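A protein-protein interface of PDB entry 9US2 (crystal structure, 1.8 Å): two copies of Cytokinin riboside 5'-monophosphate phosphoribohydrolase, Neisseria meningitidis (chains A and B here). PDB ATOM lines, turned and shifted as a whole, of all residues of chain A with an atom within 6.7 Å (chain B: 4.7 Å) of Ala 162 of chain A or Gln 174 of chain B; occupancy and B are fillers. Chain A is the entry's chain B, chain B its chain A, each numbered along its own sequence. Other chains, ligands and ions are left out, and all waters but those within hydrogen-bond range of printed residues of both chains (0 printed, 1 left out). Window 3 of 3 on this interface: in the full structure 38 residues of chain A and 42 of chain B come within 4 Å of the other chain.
No position is printed for both chains.
Among the printed residues, pairs that only touch across the chains: Phe 163 of chain A with Leu 175 of chain B (3.6 Å), Gly 166 of chain A with Trp 170 of chain B (3.6 Å), Phe 163 of chain A with Leu 180 of chain B (3.6 Å), Phe 163 of chain A with Arg 178 of chain B (3.7 Å), Gly 131 of chain A with Leu 175 of chain B (3.7 Å), Phe 163 of chain A with Gln 174 of chain B (3.7 Å), Ala 162 of chain A with Gln 174 of chain B (3.7 Å) and Gly 131 of chain A with Leu 180 of chain B (3.9 Å).
Ala 162 of chain A touches just one residue of chain B: Gln 174 (3.7 Å). Printed residues of chain B within 4 Å of Gly 131 of chain A: Leu 175 (3.7 Å) and Leu 180 (3.9 Å). Of the printed residues of chain A, Leu 175 of chain B touches Gly 131 and Phe 163. Printed residues of chain B within 4 Å of Phe 163 of chain A: Trp 170 (2.8 Å), Gln 174 (3.7 Å), Leu 175 (3.6 Å), Arg 178 (3.7 Å) and Leu 180 (3.6 Å).
OE1 of Gln 174 of chain B sits at hydrogen-bond distance from NE of Arg 178 of chain B, at 2.7 Å. The backbone NH (N) of Leu 180 of chain B is in hydrogen-bond range of the backbone carbonyl oxygen (O) of Leu 175 of chain B (2.9 Å).
Of the 10 printed residues of chain B, 5 touch a printed residue of chain A. Printed residues of chain B that touch a printed residue of chain A: Trp 170, Gln 174, Leu 175, Arg 178 and Leu 180. Hydrophobic or aromatic side chains of chain A within 4 Å of the printed part of chain B: Phe 163 and Leu 167. Among the printed residues, 10 pairs touch across the chains.
N of Leu 167 of chain A lies close to NE1 of Trp 170 of chain B (3.5 Å). The backbone carbonyl oxygen of Phe 163 of chain A lies within hydrogen-bond range of the indole nitrogen of Trp 170 of chain B (2.8 Å).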
ATOM      1  N   GLY A 131      -7.781  17.774   7.130  1.00  0.00           N
ATOM      2  CA  GLY A 131      -6.915  16.621   6.970  1.00  0.00           C
ATOM      3  C   GLY A 131      -7.304  15.803   5.756  1.00  0.00           C
ATOM      4  O   GLY A 131      -8.250  16.120   5.024  1.00  0.00           O
ATOM      5  N   VAL A 159     -13.178  22.575  11.969  1.00  0.00           N
ATOM      6  CA  VAL A 159     -12.539  23.891  11.997  1.00  0.00           C
ATOM      7  C   VAL A 159     -12.134  24.276  10.585  1.00  0.00           C
ATOM      8  O   VAL A 159     -11.363  23.565   9.932  1.00  0.00           O
ATOM      9  CB  VAL A 159     -11.326  23.908  12.938  1.00  0.00           C
ATOM     10  CG1 VAL A 159     -10.712  25.325  12.974  1.00  0.00           C
ATOM     11  CG2 VAL A 159     -11.751  23.461  14.308  1.00  0.00           C
ATOM     12  N   GLY A 160     -12.644  25.417  10.115  1.00  0.00           N
ATOM     13  CA  GLY A 160     -12.314  25.887   8.789  1.00  0.00           C
ATOM     14  C   GLY A 160     -13.559  25.932   7.928  1.00  0.00           C
ATOM     15  O   GLY A 160     -13.850  24.973   7.208  1.00  0.00           O
ATOM     16  N   LYS A 161     -14.318  27.028   8.003  1.00  0.00           N
ATOM     17  CA  LYS A 161     -15.559  27.116   7.239  1.00  0.00           C
ATOM     18  C   LYS A 161     -15.310  26.944   5.741  1.00  0.00           C
ATOM     19  O   LYS A 161     -16.060  26.242   5.056  1.00  0.00           O
ATOM     20  CB  LYS A 161     -16.238  28.454   7.514  1.00  0.00           C
ATOM     21  CG  LYS A 161     -17.064  28.453   8.772  1.00  0.00           C
ATOM     22  CD  LYS A 161     -17.522  29.857   9.137  1.00  0.00           C
ATOM     23  CE  LYS A 161     -18.504  29.808  10.283  1.00  0.00           C
ATOM     24  NZ  LYS A 161     -18.955  31.172  10.683  1.00  0.00           N
ATOM     25  N   ALA A 162     -14.252  27.567   5.210  1.00  0.00           N
ATOM     26  CA  ALA A 162     -13.973  27.424   3.782  1.00  0.00           C
ATOM     27  C   ALA A 162     -13.590  25.989   3.430  1.00  0.00           C
ATOM     28  O   ALA A 162     -14.017  25.460   2.394  1.00  0.00           O
ATOM     29  CB  ALA A 162     -12.863  28.392   3.359  1.00  0.00           C
ATOM     30  N   PHE A 163     -12.786  25.344   4.275  1.00  0.00           N
ATOM     31  CA  PHE A 163     -12.349  23.988   3.966  1.00  0.00           C
ATOM     32  C   PHE A 163     -13.510  23.005   3.994  1.00  0.00           C
ATOM     33  O   PHE A 163     -13.618  22.144   3.110  1.00  0.00           O
ATOM     34  CB  PHE A 163     -11.272  23.536   4.947  1.00  0.00           C
ATOM     35  CG  PHE A 163     -10.836  22.115   4.733  1.00  0.00           C
ATOM     36  CD1 PHE A 163      -9.905  21.815   3.756  1.00  0.00           C
ATOM     37  CD2 PHE A 163     -11.382  21.079   5.474  1.00  0.00           C
ATOM     38  CE1 PHE A 163      -9.507  20.533   3.536  1.00  0.00           C
ATOM     39  CE2 PHE A 163     -10.986  19.775   5.256  1.00  0.00           C
ATOM     40  CZ  PHE A 163     -10.047  19.493   4.279  1.00  0.00           C
ATOM     41  N   TRP A 164     -14.377  23.103   5.006  1.00  0.00           N
ATOM     42  CA  TRP A 164     -15.395  22.079   5.232  1.00  0.00           C
ATOM     43  C   TRP A 164     -16.720  22.343   4.518  1.00  0.00           C
ATOM     44  O   TRP A 164     -17.507  21.402   4.351  1.00  0.00           O
ATOM     45  CB  TRP A 164     -15.663  21.913   6.742  1.00  0.00           C
ATOM     46  CG  TRP A 164     -14.494  21.329   7.482  1.00  0.00           C
ATOM     47  CD1 TRP A 164     -13.628  21.994   8.314  1.00  0.00           C
ATOM     48  CD2 TRP A 164     -14.078  19.953   7.488  1.00  0.00           C
ATOM     49  NE1 TRP A 164     -12.689  21.110   8.833  1.00  0.00           N
ATOM     50  CE2 TRP A 164     -12.944  19.856   8.337  1.00  0.00           C
ATOM     51  CE3 TRP A 164     -14.554  18.793   6.864  1.00  0.00           C
ATOM     52  CZ2 TRP A 164     -12.282  18.648   8.573  1.00  0.00           C
ATOM     53  CZ3 TRP A 164     -13.887  17.592   7.088  1.00  0.00           C
ATOM     54  CH2 TRP A 164     -12.758  17.531   7.938  1.00  0.00           C
ATOM     55  N   SER A 165     -16.993  23.585   4.097  1.00  0.00           N
ATOM     56  CA  SER A 165     -18.349  23.924   3.658  1.00  0.00           C
ATOM     57  C   SER A 165     -18.775  23.088   2.456  1.00  0.00           C
ATOM     58  O   SER A 165     -19.943  22.706   2.348  1.00  0.00           O
ATOM     59  CB  SER A 165     -18.458  25.414   3.331  1.00  0.00           C
ATOM     60  OG  SER A 165     -17.529  25.781   2.328  1.00  0.00           O
ATOM     61  N   GLY A 166     -17.842  22.799   1.541  1.00  0.00           N
ATOM     62  CA  GLY A 166     -18.179  21.992   0.375  1.00  0.00           C
ATOM     63  C   GLY A 166     -18.636  20.587   0.735  1.00  0.00           C
ATOM     64  O   GLY A 166     -19.548  20.032   0.106  1.00  0.00           O
ATOM     65  N   LEU A 167     -17.997  19.983   1.740  1.00  0.00           N
ATOM     66  CA  LEU A 167     -18.418  18.658   2.184  1.00  0.00           C
ATOM     67  C   LEU A 167     -19.791  18.714   2.839  1.00  0.00           C
ATOM     68  O   LEU A 167     -20.651  17.868   2.567  1.00  0.00           O
ATOM     69  CB  LEU A 167     -17.374  18.078   3.140  1.00  0.00           C
ATOM     70  CG  LEU A 167     -17.687  16.697   3.714  1.00  0.00           C
ATOM     71  CD1 LEU A 167     -17.685  15.691   2.570  1.00  0.00           C
ATOM     72  CD2 LEU A 167     -16.609  16.312   4.739  1.00  0.00           C
ATOM     73  N   ILE A 191     -19.496  23.666  12.383  1.00  0.00           N
ATOM     74  CA  ILE A 191     -18.347  24.180  11.643  1.00  0.00           C
ATOM     75  C   ILE A 191     -18.041  25.588  12.145  1.00  0.00           C
ATOM     76  O   ILE A 191     -18.954  26.413  12.292  1.00  0.00           O
ATOM     77  CB  ILE A 191     -18.600  24.171  10.123  1.00  0.00           C
ATOM     78  CG1 ILE A 191     -19.061  22.774   9.659  1.00  0.00           C
ATOM     79  CG2 ILE A 191     -17.357  24.563   9.389  1.00  0.00           C
ATOM     80  CD1 ILE A 191     -19.362  22.699   8.162  1.00  0.00           C
ATOM     81  N   ASP A 193     -14.586  28.766  12.672  1.00  0.00           N
ATOM     82  CA  ASP A 193     -13.151  29.026  12.760  1.00  0.00           C
ATOM     83  C   ASP A 193     -12.835  30.161  13.718  1.00  0.00           C
ATOM     84  O   ASP A 193     -11.800  30.823  13.589  1.00  0.00           O
ATOM     85  CB  ASP A 193     -12.511  29.256  11.390  1.00  0.00           C
ATOM     86  CG  ASP A 193     -13.408  29.966  10.433  1.00  0.00           C
ATOM     87  OD1 ASP A 193     -14.247  30.770  10.885  1.00  0.00           O
ATOM     88  OD2 ASP A 193     -13.287  29.685   9.225  1.00  0.00           O
ATOM     89  N   TRP B 170     -14.815  18.145  -4.190  1.00  0.00           N
ATOM     90  CA  TRP B 170     -14.349  18.702  -2.924  1.00  0.00           C
ATOM     91  C   TRP B 170     -12.969  18.156  -2.566  1.00  0.00           C
ATOM     92  O   TRP B 170     -12.089  18.914  -2.128  1.00  0.00           O
ATOM     93  CB  TRP B 170     -15.382  18.421  -1.818  1.00  0.00           C
ATOM     94  CG  TRP B 170     -14.963  18.921  -0.452  1.00  0.00           C
ATOM     95  CD1 TRP B 170     -15.059  20.204   0.023  1.00  0.00           C
ATOM     96  CD2 TRP B 170     -14.378  18.145   0.608  1.00  0.00           C
ATOM     97  NE1 TRP B 170     -14.583  20.276   1.319  1.00  0.00           N
ATOM     98  CE2 TRP B 170     -14.150  19.030   1.700  1.00  0.00           C
ATOM     99  CE3 TRP B 170     -14.048  16.790   0.753  1.00  0.00           C
ATOM    100  CZ2 TRP B 170     -13.590  18.599   2.908  1.00  0.00           C
ATOM    101  CZ3 TRP B 170     -13.474  16.360   1.956  1.00  0.00           C
ATOM    102  CH2 TRP B 170     -13.257  17.264   3.017  1.00  0.00           C
ATOM    103  N   ILE B 171     -12.757  16.848  -2.763  1.00  0.00           N
ATOM    104  CA  ILE B 171     -11.439  16.255  -2.536  1.00  0.00           C
ATOM    105  C   ILE B 171     -10.384  16.957  -3.383  1.00  0.00           C
ATOM    106  O   ILE B 171      -9.267  17.223  -2.919  1.00  0.00           O
ATOM    107  CB  ILE B 171     -11.480  14.744  -2.835  1.00  0.00           C
ATOM    108  CG1 ILE B 171     -12.286  14.002  -1.758  1.00  0.00           C
ATOM    109  CG2 ILE B 171     -10.068  14.154  -2.956  1.00  0.00           C
ATOM    110  CD1 ILE B 171     -12.475  12.510  -2.072  1.00  0.00           C
ATOM    111  N   ASN B 172     -10.713  17.252  -4.645  1.00  0.00           N
ATOM    112  CA  ASN B 172      -9.734  17.879  -5.539  1.00  0.00           C
ATOM    113  C   ASN B 172      -9.479  19.330  -5.148  1.00  0.00           C
ATOM    114  O   ASN B 172      -8.326  19.782  -5.137  1.00  0.00           O
ATOM    115  CB  ASN B 172     -10.221  17.812  -6.986  1.00  0.00           C
ATOM    116  CG  ASN B 172     -10.017  16.454  -7.626  1.00  0.00           C
ATOM    117  OD1 ASN B 172      -9.298  15.589  -7.116  1.00  0.00           O
ATOM    118  ND2 ASN B 172     -10.661  16.258  -8.767  1.00  0.00           N
ATOM    119  N   ALA B 173     -10.544  20.077  -4.831  1.00  0.00           N
ATOM    120  CA  ALA B 173     -10.400  21.505  -4.563  1.00  0.00           C
ATOM    121  C   ALA B 173      -9.805  21.781  -3.184  1.00  0.00           C
ATOM    122  O   ALA B 173      -9.085  22.772  -3.009  1.00  0.00           O
ATOM    123  CB  ALA B 173     -11.758  22.203  -4.679  1.00  0.00           C
ATOM    124  N   GLN B 174     -10.088  20.933  -2.198  1.00  0.00           N
ATOM    125  CA  GLN B 174      -9.661  21.188  -0.829  1.00  0.00           C
ATOM    126  C   GLN B 174      -8.547  20.269  -0.343  1.00  0.00           C
ATOM    127  O   GLN B 174      -7.594  20.741   0.269  1.00  0.00           O
ATOM    128  CB  GLN B 174     -10.871  21.105   0.118  1.00  0.00           C
ATOM    129  CG  GLN B 174     -12.006  22.091  -0.228  1.00  0.00           C
ATOM    130  CD  GLN B 174     -11.575  23.554  -0.103  1.00  0.00           C
ATOM    131  OE1 GLN B 174     -10.603  23.877   0.582  1.00  0.00           O
ATOM    132  NE2 GLN B 174     -12.294  24.436  -0.775  1.00  0.00           N
ATOM    133  N   LEU B 175      -8.644  18.962  -0.558  1.00  0.00           N
ATOM    134  CA  LEU B 175      -7.585  18.072  -0.080  1.00  0.00           C
ATOM    135  C   LEU B 175      -6.363  18.118  -0.988  1.00  0.00           C
ATOM    136  O   LEU B 175      -5.245  18.364  -0.523  1.00  0.00           O
ATOM    137  CB  LEU B 175      -8.105  16.634   0.027  1.00  0.00           C
ATOM    138  CG  LEU B 175      -8.762  16.264   1.370  1.00  0.00           C
ATOM    139  CD1 LEU B 175      -9.996  17.089   1.632  1.00  0.00           C
ATOM    140  CD2 LEU B 175      -9.121  14.779   1.371  1.00  0.00           C
ATOM    141  N   LEU B 176      -6.559  17.886  -2.291  1.00  0.00           N
ATOM    142  CA  LEU B 176      -5.427  17.802  -3.213  1.00  0.00           C
ATOM    143  C   LEU B 176      -4.769  19.164  -3.424  1.00  0.00           C
ATOM    144  O   LEU B 176      -3.534  19.275  -3.417  1.00  0.00           O
ATOM    145  CB  LEU B 176      -5.877  17.221  -4.559  1.00  0.00           C
ATOM    146  CG  LEU B 176      -4.794  17.095  -5.643  1.00  0.00           C
ATOM    147  CD1 LEU B 176      -3.724  16.076  -5.257  1.00  0.00           C
ATOM    148  CD2 LEU B 176      -5.398  16.742  -6.997  1.00  0.00           C
ATOM    149  N   ALA B 177      -5.576  20.207  -3.627  1.00  0.00           N
ATOM    150  CA  ALA B 177      -5.018  21.528  -3.913  1.00  0.00           C
ATOM    151  C   ALA B 177      -4.299  22.122  -2.706  1.00  0.00           C
ATOM    152  O   ALA B 177      -3.411  22.965  -2.875  1.00  0.00           O
ATOM    153  CB  ALA B 177      -6.121  22.473  -4.391  1.00  0.00           C
ATOM    154  N   ARG B 178      -4.665  21.719  -1.489  1.00  0.00           N
ATOM    155  CA  ARG B 178      -3.957  22.189  -0.304  1.00  0.00           C
ATOM    156  C   ARG B 178      -2.817  21.265   0.094  1.00  0.00           C
ATOM    157  O   ARG B 178      -2.160  21.511   1.111  1.00  0.00           O
ATOM    158  CB  ARG B 178      -4.919  22.356   0.874  1.00  0.00           C
ATOM    159  CG  ARG B 178      -6.038  23.356   0.640  1.00  0.00           C
ATOM    160  CD  ARG B 178      -6.947  23.414   1.848  1.00  0.00           C
ATOM    161  NE  ARG B 178      -8.130  24.233   1.626  1.00  0.00           N
ATOM    162  CZ  ARG B 178      -8.189  25.542   1.843  1.00  0.00           C
ATOM    163  NH1 ARG B 178      -7.122  26.228   2.236  1.00  0.00           N
ATOM    164  NH2 ARG B 178      -9.340  26.183   1.644  1.00  0.00           N
ATOM    165  N   LEU B 180      -2.947  18.164   1.174  1.00  0.00           N
ATOM    166  CA  LEU B 180      -3.225  17.220   2.253  1.00  0.00           C
ATOM    167  C   LEU B 180      -3.188  15.773   1.786  1.00  0.00           C
ATOM    168  O   LEU B 180      -3.022  14.863   2.614  1.00  0.00           O
ATOM    169  CB  LEU B 180      -4.580  17.546   2.869  1.00  0.00           C
ATOM    170  CG  LEU B 180      -4.720  18.998   3.319  1.00  0.00           C
ATOM    171  CD1 LEU B 180      -6.122  19.266   3.883  1.00  0.00           C
ATOM    172  CD2 LEU B 180      -3.646  19.367   4.341  1.00  0.00           C
